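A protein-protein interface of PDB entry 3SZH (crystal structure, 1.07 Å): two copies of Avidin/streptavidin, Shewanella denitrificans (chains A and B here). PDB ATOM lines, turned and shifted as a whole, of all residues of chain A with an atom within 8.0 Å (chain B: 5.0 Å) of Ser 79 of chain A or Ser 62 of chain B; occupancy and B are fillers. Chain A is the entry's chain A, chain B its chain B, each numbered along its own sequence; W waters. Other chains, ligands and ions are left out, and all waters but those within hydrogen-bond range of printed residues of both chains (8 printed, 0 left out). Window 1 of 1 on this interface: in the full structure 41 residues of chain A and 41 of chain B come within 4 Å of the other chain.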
ATOM      1  N   ASN A  53      24.643 -27.915   9.887  1.00  0.00           N
ATOM      2  CA  ASN A  53      23.765 -28.947  10.457  1.00  0.00           C
ATOM      3  C   ASN A  53      23.080 -28.393  11.700  1.00  0.00           C
ATOM      4  O   ASN A  53      23.345 -27.269  12.126  1.00  0.00           O
ATOM      5  CB  ASN A  53      24.516 -30.281  10.706  1.00  0.00           C
ATOM      6  CG  ASN A  53      25.690 -30.148  11.650  1.00  0.00           C
ATOM      7  OD1 ASN A  53      25.739 -29.242  12.492  1.00  0.00           O
ATOM      8  ND2 ASN A  53      26.657 -31.069  11.529  1.00  0.00           N
ATOM      9  N   SER A  62      18.576 -25.105  16.574  1.00  0.00           N
ATOM     10  CA  SER A  62      20.025 -24.921  16.701  1.00  0.00           C
ATOM     11  C   SER A  62      20.615 -25.179  15.338  1.00  0.00           C
ATOM     12  O   SER A  62      20.132 -26.048  14.593  1.00  0.00           O
ATOM     13  CB  SER A  62      20.647 -25.867  17.737  1.00  0.00           C
ATOM     14  OG  SER A  62      20.742 -27.188  17.226  1.00  0.00           O
ATOM     15  N   PHE A  63      21.656 -24.436  14.984  1.00  0.00           N
ATOM     16  CA  PHE A  63      22.393 -24.727  13.767  1.00  0.00           C
ATOM     17  C   PHE A  63      23.846 -24.349  13.972  1.00  0.00           C
ATOM     18  O   PHE A  63      24.161 -23.453  14.769  1.00  0.00           O
ATOM     19  CB  PHE A  63      21.776 -24.106  12.499  1.00  0.00           C
ATOM     20  CG  PHE A  63      21.616 -22.609  12.542  1.00  0.00           C
ATOM     21  CD1 PHE A  63      20.481 -22.035  13.126  1.00  0.00           C
ATOM     22  CD2 PHE A  63      22.552 -21.767  11.946  1.00  0.00           C
ATOM     23  CE1 PHE A  63      20.321 -20.651  13.134  1.00  0.00           C
ATOM     24  CE2 PHE A  63      22.386 -20.397  11.966  1.00  0.00           C
ATOM     25  CZ  PHE A  63      21.265 -19.842  12.535  1.00  0.00           C
ATOM     26  N   SER A  64      24.740 -25.030  13.251  1.00  0.00           N
ATOM     27  CA  SER A  64      26.175 -24.848  13.452  1.00  0.00           C
ATOM     28  C   SER A  64      26.879 -25.029  12.119  1.00  0.00           C
ATOM     29  O   SER A  64      26.486 -25.849  11.292  1.00  0.00           O
ATOM     30  CB  SER A  64      26.678 -25.832  14.526  1.00  0.00           C
ATOM     31  OG  SER A  64      28.088 -25.749  14.773  1.00  0.00           O
ATOM     32  N   THR A  65      27.942 -24.234  11.943  1.00  0.00           N
ATOM     33  CA  THR A  65      28.757 -24.321  10.748  1.00  0.00           C
ATOM     34  C   THR A  65      30.242 -24.313  11.117  1.00  0.00           C
ATOM     35  O   THR A  65      30.679 -23.568  11.985  1.00  0.00           O
ATOM     36  CB  THR A  65      28.392 -23.208   9.725  1.00  0.00           C
ATOM     37  OG1 THR A  65      28.998 -23.507   8.460  1.00  0.00           O
ATOM     38  CG2 THR A  65      28.794 -21.807  10.170  1.00  0.00           C
ATOM     39  N   LYS A  66      31.007 -25.193  10.469  1.00  0.00           N
ATOM     40  CA  LYS A  66      32.460 -25.191  10.537  1.00  0.00           C
ATOM     41  C   LYS A  66      32.961 -24.276   9.421  1.00  0.00           C
ATOM     42  O   LYS A  66      32.594 -24.421   8.256  1.00  0.00           O
ATOM     43  CB  LYS A  66      32.961 -26.623  10.359  1.00  0.00           C
ATOM     44  CG  LYS A  66      34.476 -26.753  10.195  1.00  0.00           C
ATOM     45  CD  LYS A  66      34.901 -28.215  10.164  1.00  0.00           C
ATOM     46  CE  LYS A  66      36.367 -28.348   9.772  1.00  0.00           C
ATOM     47  NZ  LYS A  66      36.847 -29.737   9.910  1.00  0.00           N
ATOM     48  N   TRP A  67      33.856 -23.352   9.772  1.00  0.00           N
ATOM     49  CA  TRP A  67      34.362 -22.388   8.799  1.00  0.00           C
ATOM     50  C   TRP A  67      35.516 -22.964   7.976  1.00  0.00           C
ATOM     51  O   TRP A  67      36.665 -22.493   8.025  1.00  0.00           O
ATOM     52  CB  TRP A  67      34.780 -21.096   9.495  1.00  0.00           C
ATOM     53  CG  TRP A  67      33.617 -20.413  10.181  1.00  0.00           C
ATOM     54  CD1 TRP A  67      33.392 -20.341  11.511  1.00  0.00           C
ATOM     55  CD2 TRP A  67      32.512 -19.759   9.541  1.00  0.00           C
ATOM     56  NE1 TRP A  67      32.215 -19.642  11.765  1.00  0.00           N
ATOM     57  CE2 TRP A  67      31.654 -19.287  10.564  1.00  0.00           C
ATOM     58  CE3 TRP A  67      32.186 -19.506   8.203  1.00  0.00           C
ATOM     59  CZ2 TRP A  67      30.475 -18.568  10.286  1.00  0.00           C
ATOM     60  CZ3 TRP A  67      31.021 -18.818   7.924  1.00  0.00           C
ATOM     61  CH2 TRP A  67      30.186 -18.343   8.959  1.00  0.00           C
ATOM     62  N   SER A  76      37.643 -22.206  12.763  1.00  0.00           N
ATOM     63  CA  SER A  76      36.693 -22.048  13.870  1.00  0.00           C
ATOM     64  C   SER A  76      35.340 -22.633  13.501  1.00  0.00           C
ATOM     65  O   SER A  76      35.124 -23.047  12.358  1.00  0.00           O
ATOM     66  CB  SER A  76      36.518 -20.592  14.251  1.00  0.00           C
ATOM     67  OG  SER A  76      36.209 -19.795  13.143  1.00  0.00           O
ATOM     68  N   ILE A  77      34.455 -22.660  14.498  1.00  0.00           N
ATOM     69  CA  ILE A  77      33.093 -23.185  14.371  1.00  0.00           C
ATOM     70  C   ILE A  77      32.146 -22.223  15.076  1.00  0.00           C
ATOM     71  O   ILE A  77      32.386 -21.826  16.218  1.00  0.00           O
ATOM     72  CB  ILE A  77      32.972 -24.580  15.049  1.00  0.00           C
ATOM     73  CG1 ILE A  77      33.982 -25.592  14.482  1.00  0.00           C
ATOM     74  CG2 ILE A  77      31.547 -25.117  14.910  1.00  0.00           C
ATOM     75  CD1 ILE A  77      34.152 -26.790  15.357  1.00  0.00           C
ATOM     76  N   THR A  78      31.035 -21.869  14.411  1.00  0.00           N
ATOM     77  CA  THR A  78      29.978 -21.062  15.048  1.00  0.00           C
ATOM     78  C   THR A  78      28.741 -21.928  15.262  1.00  0.00           C
ATOM     79  O   THR A  78      28.380 -22.730  14.400  1.00  0.00           O
ATOM     80  CB  THR A  78      29.629 -19.818  14.242  1.00  0.00           C
ATOM     81  OG1 THR A  78      30.820 -19.028  14.130  1.00  0.00           O
ATOM     82  CG2 THR A  78      28.534 -18.991  14.901  1.00  0.00           C
ATOM     83  N   SER A  79      28.143 -21.784  16.435  1.00  0.00           N
ATOM     84  CA  SER A  79      26.880 -22.434  16.779  1.00  0.00           C
ATOM     85  C   SER A  79      25.870 -21.407  17.234  1.00  0.00           C
ATOM     86  O   SER A  79      26.169 -20.583  18.086  1.00  0.00           O
ATOM     87  CB  SER A  79      27.105 -23.430  17.898  1.00  0.00           C
ATOM     88  OG  SER A  79      28.005 -24.429  17.475  1.00  0.00           O
ATOM     89  N   TRP A  80      24.667 -21.512  16.685  1.00  0.00           N
ATOM     90  CA  TRP A  80      23.528 -20.653  17.032  1.00  0.00           C
ATOM     91  C   TRP A  80      22.468 -21.479  17.745  1.00  0.00           C
ATOM     92  O   TRP A  80      22.180 -22.615  17.353  1.00  0.00           O
ATOM     93  CB  TRP A  80      22.893 -20.064  15.772  1.00  0.00           C
ATOM     94  CG  TRP A  80      23.704 -19.077  14.981  1.00  0.00           C
ATOM     95  CD1 TRP A  80      23.541 -17.718  14.993  1.00  0.00           C
ATOM     96  CD2 TRP A  80      24.731 -19.340  13.997  1.00  0.00           C
ATOM     97  NE1 TRP A  80      24.379 -17.123  14.091  1.00  0.00           N
ATOM     98  CE2 TRP A  80      25.112 -18.092  13.450  1.00  0.00           C
ATOM     99  CE3 TRP A  80      25.323 -20.517  13.480  1.00  0.00           C
ATOM    100  CZ2 TRP A  80      26.063 -17.976  12.418  1.00  0.00           C
ATOM    101  CZ3 TRP A  80      26.234 -20.398  12.443  1.00  0.00           C
ATOM    102  CH2 TRP A  80      26.599 -19.144  11.929  1.00  0.00           C
ATOM    103  N   SER A  81      21.893 -20.894  18.780  1.00  0.00           N
ATOM    104  CA  SER A  81      20.711 -21.437  19.458  1.00  0.00           C
ATOM    105  C   SER A  81      19.641 -20.364  19.409  1.00  0.00           C
ATOM    106  O   SER A  81      19.895 -19.213  19.709  1.00  0.00           O
ATOM    107  CB  SER A  81      20.990 -21.763  20.929  1.00  0.00           C
ATOM    108  OG  SER A  81      22.016 -22.733  21.044  1.00  0.00           O
ATOM    109  N   GLY A  82      18.437 -20.713  19.005  1.00  0.00           N
ATOM    110  CA  GLY A  82      17.400 -19.707  18.972  1.00  0.00           C
ATOM    111  C   GLY A  82      16.005 -20.220  18.757  1.00  0.00           C
ATOM    112  O   GLY A  82      15.718 -21.405  18.928  1.00  0.00           O
ATOM    113  N   THR A  95      18.450 -15.430  17.858  1.00  0.00           N
ATOM    114  CA  THR A  95      19.497 -16.384  18.249  1.00  0.00           C
ATOM    115  C   THR A  95      20.554 -15.764  19.145  1.00  0.00           C
ATOM    116  O   THR A  95      20.784 -14.541  19.142  1.00  0.00           O
ATOM    117  CB  THR A  95      20.286 -16.983  17.037  1.00  0.00           C
ATOM    118  OG1 THR A  95      21.129 -15.985  16.451  1.00  0.00           O
ATOM    119  CG2 THR A  95      19.368 -17.564  15.992  1.00  0.00           C
ATOM    120  N   LEU A  96      21.229 -16.648  19.875  1.00  0.00           N
ATOM    121  CA  LEU A  96      22.501 -16.362  20.537  1.00  0.00           C
ATOM    122  C   LEU A  96      23.514 -17.329  19.961  1.00  0.00           C
ATOM    123  O   LEU A  96      23.239 -18.540  19.844  1.00  0.00           O
ATOM    124  CB  LEU A  96      22.365 -16.572  22.042  1.00  0.00           C
ATOM    125  CG  LEU A  96      21.334 -15.667  22.732  1.00  0.00           C
ATOM    126  CD1 LEU A  96      21.292 -15.972  24.218  1.00  0.00           C
ATOM    127  CD2 LEU A  96      21.628 -14.196  22.497  1.00  0.00           C
ATOM    128  N   TRP A  97      24.687 -16.820  19.592  1.00  0.00           N
ATOM    129  CA  TRP A  97      25.714 -17.656  19.004  1.00  0.00           C
ATOM    130  C   TRP A  97      26.983 -17.683  19.833  1.00  0.00           C
ATOM    131  O   TRP A  97      27.256 -16.780  20.651  1.00  0.00           O
ATOM    132  CB  TRP A  97      26.046 -17.241  17.563  1.00  0.00           C
ATOM    133  CG  TRP A  97      26.445 -15.815  17.347  1.00  0.00           C
ATOM    134  CD1 TRP A  97      25.641 -14.808  16.917  1.00  0.00           C
ATOM    135  CD2 TRP A  97      27.748 -15.231  17.544  1.00  0.00           C
ATOM    136  NE1 TRP A  97      26.340 -13.628  16.832  1.00  0.00           N
ATOM    137  CE2 TRP A  97      27.647 -13.864  17.191  1.00  0.00           C
ATOM    138  CE3 TRP A  97      29.002 -15.739  17.939  1.00  0.00           C
ATOM    139  CZ2 TRP A  97      28.744 -12.990  17.256  1.00  0.00           C
ATOM    140  CZ3 TRP A  97      30.101 -14.863  17.997  1.00  0.00           C
ATOM    141  CH2 TRP A  97      29.960 -13.508  17.663  1.00  0.00           C
ATOM    142  N   GLN A  98      27.762 -18.746  19.607  1.00  0.00           N
ATOM    143  CA  GLN A  98      29.085 -18.932  20.200  1.00  0.00           C
ATOM    144  C   GLN A  98      30.028 -19.361  19.088  1.00  0.00           C
ATOM    145  O   GLN A  98      29.681 -20.211  18.259  1.00  0.00           O
ATOM    146  CB  GLN A  98      29.046 -20.027  21.241  1.00  0.00           C
ATOM    147  CG  GLN A  98      28.078 -19.732  22.409  1.00  0.00           C
ATOM    148  CD  GLN A  98      28.150 -20.739  23.541  1.00  0.00           C
ATOM    149  OE1 GLN A  98      28.169 -21.945  23.339  1.00  0.00           O
ATOM    150  NE2 GLN A  98      28.204 -20.232  24.753  1.00  0.00           N
ATOM    151  N   LEU A  99      31.225 -18.797  19.100  1.00  0.00           N
ATOM    152  CA  LEU A  99      32.277 -19.067  18.133  1.00  0.00           C
ATOM    153  C   LEU A  99      33.478 -19.624  18.891  1.00  0.00           C
ATOM    154  O   LEU A  99      33.986 -18.947  19.799  1.00  0.00           O
ATOM    155  CB  LEU A  99      32.659 -17.741  17.481  1.00  0.00           C
ATOM    156  CG  LEU A  99      33.875 -17.585  16.558  1.00  0.00           C
ATOM    157  CD1 LEU A  99      35.237 -17.676  17.246  1.00  0.00           C
ATOM    158  CD2 LEU A  99      33.787 -18.550  15.393  1.00  0.00           C
ATOM    159  N   VAL A 100      33.916 -20.831  18.553  1.00  0.00           N
ATOM    160  CA  VAL A 100      35.098 -21.437  19.149  1.00  0.00           C
ATOM    161  C   VAL A 100      36.165 -21.606  18.081  1.00  0.00           C
ATOM    162  O   VAL A 100      35.908 -22.104  16.971  1.00  0.00           O
ATOM    163  CB  VAL A 100      34.777 -22.757  19.901  1.00  0.00           C
ATOM    164  CG1 VAL A 100      34.174 -23.851  18.986  1.00  0.00           C
ATOM    165  CG2 VAL A 100      36.020 -23.281  20.635  1.00  0.00           C
ATOM    166  N   LEU A 111      33.871 -16.717  21.635  1.00  0.00           N
ATOM    167  CA  LEU A 111      33.219 -15.441  21.391  1.00  0.00           C
ATOM    168  C   LEU A 111      31.705 -15.643  21.351  1.00  0.00           C
ATOM    169  O   LEU A 111      31.220 -16.687  20.944  1.00  0.00           O
ATOM    170  CB  LEU A 111      33.687 -14.859  20.069  1.00  0.00           C
ATOM    171  CG  LEU A 111      35.193 -14.678  19.926  1.00  0.00           C
ATOM    172  CD1 LEU A 111      35.500 -14.121  18.550  1.00  0.00           C
ATOM    173  CD2 LEU A 111      35.738 -13.787  21.039  1.00  0.00           C
ATOM    174  N   LYS A 112      30.966 -14.637  21.781  1.00  0.00           N
ATOM    175  CA  LYS A 112      29.511 -14.723  21.842  1.00  0.00           C
ATOM    176  C   LYS A 112      28.843 -13.491  21.261  1.00  0.00           C
ATOM    177  O   LYS A 112      29.383 -12.374  21.340  1.00  0.00           O
ATOM    178  CB  LYS A 112      29.039 -14.864  23.293  1.00  0.00           C
ATOM    179  CG  LYS A 112      29.607 -16.036  24.070  1.00  0.00           C
ATOM    180  CD  LYS A 112      28.877 -16.160  25.402  1.00  0.00           C
ATOM    181  CE  LYS A 112      29.522 -17.195  26.312  1.00  0.00           C
ATOM    182  NZ  LYS A 112      30.781 -16.674  26.920  1.00  0.00           N
ATOM    183  N   GLY A 113      27.637 -13.671  20.733  1.00  0.00           N
ATOM    184  CA  GLY A 113      26.869 -12.528  20.295  1.00  0.00           C
ATOM    185  C   GLY A 113      25.431 -12.933  20.024  1.00  0.00           C
ATOM    186  O   GLY A 113      25.009 -14.052  20.324  1.00  0.00           O
ATOM    187  N   ASP A 115      22.322 -12.759  17.012  1.00  0.00           N
ATOM    188  CA  ASP A 115      21.892 -12.513  15.618  1.00  0.00           C
ATOM    189  C   ASP A 115      20.382 -12.649  15.558  1.00  0.00           C
ATOM    190  O   ASP A 115      19.841 -13.576  16.162  1.00  0.00           O
ATOM    191  CB  ASP A 115      22.461 -13.561  14.647  1.00  0.00           C
ATOM    192  CG  ASP A 115      23.912 -13.334  14.274  1.00  0.00           C
ATOM    193  OD1 ASP A 115      24.522 -12.295  14.640  1.00  0.00           O
ATOM    194  OD2 ASP A 115      24.445 -14.250  13.601  1.00  0.00           O
ATOM    195  N   LEU B  32      30.407 -34.443  12.626  1.00  0.00           N
ATOM    196  CA  LEU B  32      30.321 -35.387  13.719  1.00  0.00           C
ATOM    197  C   LEU B  32      28.939 -36.009  13.829  1.00  0.00           C
ATOM    198  O   LEU B  32      27.921 -35.319  13.658  1.00  0.00           O
ATOM    199  CB  LEU B  32      30.667 -34.634  15.022  1.00  0.00           C
ATOM    200  CG  LEU B  32      30.587 -35.339  16.373  1.00  0.00           C
ATOM    201  CD1 LEU B  32      31.613 -34.740  17.333  1.00  0.00           C
ATOM    202  CD2 LEU B  32      29.182 -35.247  16.954  1.00  0.00           C
ATOM    203  N   ASN B  53      24.656 -34.287  16.567  1.00  0.00           N
ATOM    204  CA  ASN B  53      25.439 -33.905  15.401  1.00  0.00           C
ATOM    205  C   ASN B  53      26.371 -32.748  15.788  1.00  0.00           C
ATOM    206  O   ASN B  53      26.323 -32.263  16.911  1.00  0.00           O
ATOM    207  CB  ASN B  53      24.550 -33.591  14.171  1.00  0.00           C
ATOM    208  CG  ASN B  53      23.555 -32.492  14.422  1.00  0.00           C
ATOM    209  OD1 ASN B  53      23.762 -31.622  15.279  1.00  0.00           O
ATOM    210  ND2 ASN B  53      22.456 -32.494  13.661  1.00  0.00           N
ATOM    211  N   GLY B  54      27.244 -32.338  14.868  1.00  0.00           N
ATOM    212  CA  GLY B  54      28.179 -31.253  15.162  1.00  0.00           C
ATOM    213  C   GLY B  54      29.330 -31.244  14.198  1.00  0.00           C
ATOM    214  O   GLY B  54      29.249 -31.806  13.093  1.00  0.00           O
ATOM    215  N   TRP B  55      30.431 -30.646  14.665  1.00  0.00           N
ATOM    216  CA  TRP B  55      31.631 -30.406  13.850  1.00  0.00           C
ATOM    217  C   TRP B  55      32.868 -30.478  14.733  1.00  0.00           C
ATOM    218  O   TRP B  55      32.837 -30.059  15.900  1.00  0.00           O
ATOM    219  CB  TRP B  55      31.604 -28.989  13.250  1.00  0.00           C
ATOM    220  CG  TRP B  55      30.497 -28.750  12.276  1.00  0.00           C
ATOM    221  CD1 TRP B  55      29.365 -28.032  12.503  1.00  0.00           C
ATOM    222  CD2 TRP B  55      30.444 -29.206  10.922  1.00  0.00           C
ATOM    223  NE1 TRP B  55      28.582 -28.060  11.371  1.00  0.00           N
ATOM    224  CE2 TRP B  55      29.216 -28.773  10.387  1.00  0.00           C
ATOM    225  CE3 TRP B  55      31.314 -29.953  10.109  1.00  0.00           C
ATOM    226  CZ2 TRP B  55      28.827 -29.056   9.059  1.00  0.00           C
ATOM    227  CZ3 TRP B  55      30.938 -30.242   8.800  1.00  0.00           C
ATOM    228  CH2 TRP B  55      29.700 -29.797   8.284  1.00  0.00           C
ATOM    229  N   ALA B  60      38.908 -27.666  18.191  1.00  0.00           N
ATOM    230  CA  ALA B  60      37.600 -27.056  18.395  1.00  0.00           C
ATOM    231  C   ALA B  60      36.512 -28.082  18.066  1.00  0.00           C
ATOM    232  O   ALA B  60      36.644 -28.889  17.143  1.00  0.00           O
ATOM    233  CB  ALA B  60      37.445 -25.837  17.518  1.00  0.00           C
ATOM    234  N   ILE B  61      35.422 -28.005  18.813  1.00  0.00           N
ATOM    235  CA  ILE B  61      34.282 -28.916  18.602  1.00  0.00           C
ATOM    236  C   ILE B  61      32.986 -28.212  18.952  1.00  0.00           C
ATOM    237  O   ILE B  61      32.905 -27.426  19.913  1.00  0.00           O
ATOM    238  CB  ILE B  61      34.441 -30.228  19.435  1.00  0.00           C
ATOM    239  CG1 ILE B  61      33.262 -31.186  19.207  1.00  0.00           C
ATOM    240  CG2 ILE B  61      34.692 -29.926  20.912  1.00  0.00           C
ATOM    241  CD1 ILE B  61      33.441 -32.532  19.822  1.00  0.00           C
ATOM    242  N   SER B  62      31.960 -28.462  18.151  1.00  0.00           N
ATOM    243  CA  SER B  62      30.583 -28.136  18.507  1.00  0.00           C
ATOM    244  C   SER B  62      29.773 -29.423  18.431  1.00  0.00           C
ATOM    245  O   SER B  62      29.994 -30.256  17.535  1.00  0.00           O
ATOM    246  CB  SER B  62      29.983 -27.060  17.582  1.00  0.00           C
ATOM    247  OG  SER B  62      29.609 -27.580  16.333  1.00  0.00           O
ATOM    248  N   PHE B  63      28.823 -29.581  19.338  1.00  0.00           N
ATOM    249  CA  PHE B  63      27.866 -30.684  19.190  1.00  0.00           C
ATOM    250  C   PHE B  63      26.554 -30.265  19.774  1.00  0.00           C
ATOM    251  O   PHE B  63      26.492 -29.400  20.647  1.00  0.00           O
ATOM    252  CB  PHE B  63      28.417 -32.000  19.789  1.00  0.00           C
ATOM    253  CG  PHE B  63      28.784 -31.937  21.255  1.00  0.00           C
ATOM    254  CD1 PHE B  63      30.038 -31.518  21.661  1.00  0.00           C
ATOM    255  CD2 PHE B  63      27.862 -32.360  22.237  1.00  0.00           C
ATOM    256  CE1 PHE B  63      30.385 -31.489  23.011  1.00  0.00           C
ATOM    257  CE2 PHE B  63      28.227 -32.329  23.606  1.00  0.00           C
ATOM    258  CZ  PHE B  63      29.481 -31.906  23.972  1.00  0.00           C
ATOM    259  N   SER B  64      25.482 -30.858  19.258  1.00  0.00           N
ATOM    260  CA  SER B  64      24.134 -30.467  19.678  1.00  0.00           C
ATOM    261  C   SER B  64      23.218 -31.675  19.652  1.00  0.00           C
ATOM    262  O   SER B  64      23.360 -32.595  18.818  1.00  0.00           O
ATOM    263  CB  SER B  64      23.638 -29.330  18.778  1.00  0.00           C
ATOM    264  OG  SER B  64      22.288 -28.946  18.974  1.00  0.00           O
ATOM    265  N   SER B  79      23.089 -27.110  22.787  1.00  0.00           N
ATOM    266  CA  SER B  79      24.250 -26.994  21.921  1.00  0.00           C
ATOM    267  C   SER B  79      25.463 -26.642  22.762  1.00  0.00           C
ATOM    268  O   SER B  79      25.416 -25.728  23.580  1.00  0.00           O
ATOM    269  CB  SER B  79      24.076 -25.886  20.904  1.00  0.00           C
ATOM    270  OG  SER B  79      22.971 -26.164  20.086  1.00  0.00           O
ATOM    271  N   TRP B  80      26.553 -27.352  22.559  1.00  0.00           N
ATOM    272  CA  TRP B  80      27.841 -27.138  23.226  1.00  0.00           C
ATOM    273  C   TRP B  80      28.845 -26.629  22.205  1.00  0.00           C
ATOM    274  O   TRP B  80      28.920 -27.109  21.070  1.00  0.00           O
ATOM    275  CB  TRP B  80      28.340 -28.469  23.766  1.00  0.00           C
ATOM    276  CG  TRP B  80      27.610 -29.094  24.908  1.00  0.00           C
ATOM    277  CD1 TRP B  80      27.967 -29.052  26.218  1.00  0.00           C
ATOM    278  CD2 TRP B  80      26.436 -29.921  24.847  1.00  0.00           C
ATOM    279  NE1 TRP B  80      27.131 -29.814  26.985  1.00  0.00           N
ATOM    280  CE2 TRP B  80      26.159 -30.347  26.169  1.00  0.00           C
ATOM    281  CE3 TRP B  80      25.618 -30.390  23.799  1.00  0.00           C
ATOM    282  CZ2 TRP B  80      25.122 -31.239  26.468  1.00  0.00           C
ATOM    283  CZ3 TRP B  80      24.566 -31.252  24.105  1.00  0.00           C
ATOM    284  CH2 TRP B  80      24.338 -31.673  25.423  1.00  0.00           C
ATOM    285  N   SER B  81      29.675 -25.689  22.656  1.00  0.00           N
ATOM    286  CA  SER B  81      30.841 -25.223  21.914  1.00  0.00           C
ATOM    287  C   SER B  81      32.036 -25.378  22.828  1.00  0.00           C
ATOM    288  O   SER B  81      31.978 -24.966  23.989  1.00  0.00           O
ATOM    289  CB  SER B  81      30.726 -23.741  21.562  1.00  0.00           C
ATOM    290  OG  SER B  81      29.615 -23.495  20.716  1.00  0.00           O
ATOM    291  N   GLN B  98      24.367 -23.892  25.539  1.00  0.00           N
ATOM    292  CA  GLN B  98      23.127 -23.118  25.495  1.00  0.00           C
ATOM    293  C   GLN B  98      21.988 -24.099  25.293  1.00  0.00           C
ATOM    294  O   GLN B  98      22.070 -25.007  24.446  1.00  0.00           O
ATOM    295  CB  GLN B  98      23.164 -22.109  24.352  1.00  0.00           C
ATOM    296  CG  GLN B  98      24.347 -21.120  24.424  1.00  0.00           C
ATOM    297  CD  GLN B  98      24.271 -20.058  23.351  1.00  0.00           C
ATOM    298  OE1 GLN B  98      24.046 -20.338  22.165  1.00  0.00           O
ATOM    299  NE2 GLN B  98      24.445 -18.830  23.756  1.00  0.00           N
HETATM  300  O   HOH W   1      24.052 -24.916  17.663  1.00  0.00           O
HETATM  301  O   HOH W   2      24.951 -29.142  15.117  1.00  0.00           O
HETATM  302  O   HOH W   3      20.757 -25.099  21.366  1.00  0.00           O
HETATM  303  O   HOH W   4      25.842 -16.500  23.058  1.00  0.00           O
HETATM  304  O   HOH W   5      26.891 -23.733  21.552  1.00  0.00           O
HETATM  305  O   HOH W   6      24.765 -22.328  20.428  1.00  0.00           O
HETATM  306  O   HOH W   7      30.507 -23.418  18.158  1.00  0.00           O
HETATM  307  O   HOH W   8      26.797 -26.561  19.035  1.00  0.00           O
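ND2 of Asn 53 of chain A lies within hydrogen-bond range of O of Gly 54 of chain B.
The side-chain amide oxygen of Asn 53 of chain A is in hydrogen-bond range of the indole nitrogen of Trp 55 of chain B (3.3 Å).
The side-chain hydroxyl (OG) of Ser 64 of chain B lies within hydrogen-bond range of the side-chain hydroxyl (OG) of Ser 62 of chain A (2.9 Å).
The backbone carbonyl oxygen (O) of Ser 64 of chain A is in hydrogen-bond range of the indole nitrogen (NE1) of Trp 55 of chain B, at 3.0 Å.
The side-chain hydroxyl (OG) of Ser 64 of chain A lies within hydrogen-bond range of the side-chain hydroxyl (OG) of Ser 62 of chain B.
The side-chain amide oxygen (OE1) of Gln 98 of chain B is in hydrogen-bond range of the side-chain hydroxyl (OG) of Ser 81 of chain A (3.3 Å).
The side-chain amide oxygen (OE1) of Gln 98 of chain B sits close to the backbone carbonyl oxygen (O) of Leu 96 of chain A, 3.0 Å away.
The side-chain amide oxygen (OE1) of Gln 98 of chain A sits at hydrogen-bond distance from the side-chain hydroxyl (OG) of Ser 81 of chain B (3.4 Å).
The backbone carbonyl oxygen (O) of Ser 81 of chain A is in hydrogen-bond range of the backbone NH (N) of Leu 96 of chain A (2.9 Å).
The backbone NH (N) of Leu 32 of chain B is in hydrogen-bond range of the backbone carbonyl oxygen (O) of Gly 54 of chain B.
O of Trp 55 of chain B lies within hydrogen-bond range of N of Ser 62 of chain B (2.9 Å).
CA of Thr 65 of chain A touches NE1 of Trp 55 of chain B (3.8 Å).
Lys 66 of chain A touches Trp 55 of chain B (CB to CD2, 3.7 Å).
Ile 77 of chain A touches Ala 60 of chain B (CD1 to O, 3.7 Å).
CB of Ser 62 of chain B touches OG of Ser 79 of chain A (3.3 Å).
OG of Ser 79 of chain B touches OG of Ser 81 of chain A (3.7 Å).
Ile 61 of chain B touches Val 100 of chain A (O to CG1, 3.9 Å).
Printed residues of chain B within 4 Å of Asn 53 of chain A: Gly 54 (3.1 Å) and Trp 55 (3.3 Å).
Of the printed residues of chain A, Gly 54 of chain B touches Asn 53.
Printed residues of chain B within 4 Å of Leu 96 of chain A: Gln 98 (3.0 Å).
Lys 112 of chain A touches none of the printed residues of chain B.
The nearest printed residue of chain A that does not touch Ser 62 of chain B is Val 100 of chain A (5.2 Å).
The nearest printed residue of chain B that does not touch Lys 66 of chain A is Ser 62 of chain B (6.5 Å).
Among the printed residues, 20 pairs touch across the chains.
Ser 62 of chain A touches Ser 79 of chain B, and with the chains exchanged Ser 79 of chain A touches Ser 62 of chain B.
Ser 81 of chain A touches Gln 98 of chain B, and with the chains exchanged Gln 98 of chain A touches Ser 81 of chain B.
Gln 98 of chain B touches its own counterpart, Gln 98 of chain A.
Positions printed for both chains: 53, 62, 63, 64, 79, 80, 81 and 98.
Water W2 bridges OD1 of Asn 53 of chain A and OD1 of Asn 53 of chain B.
Water W4 lies within hydrogen-bond range of NE2 of Gln 98 of chain B (2.8 Å) and O of Trp 97 of chain A (2.8 Å).
Water W8 lies within hydrogen-bond range of the side-chain hydroxyl of Ser 79 of chain A, the backbone carbonyl oxygen of Trp 80 of chain B and the backbone carbonyl oxygen of Phe 63 of chain B.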
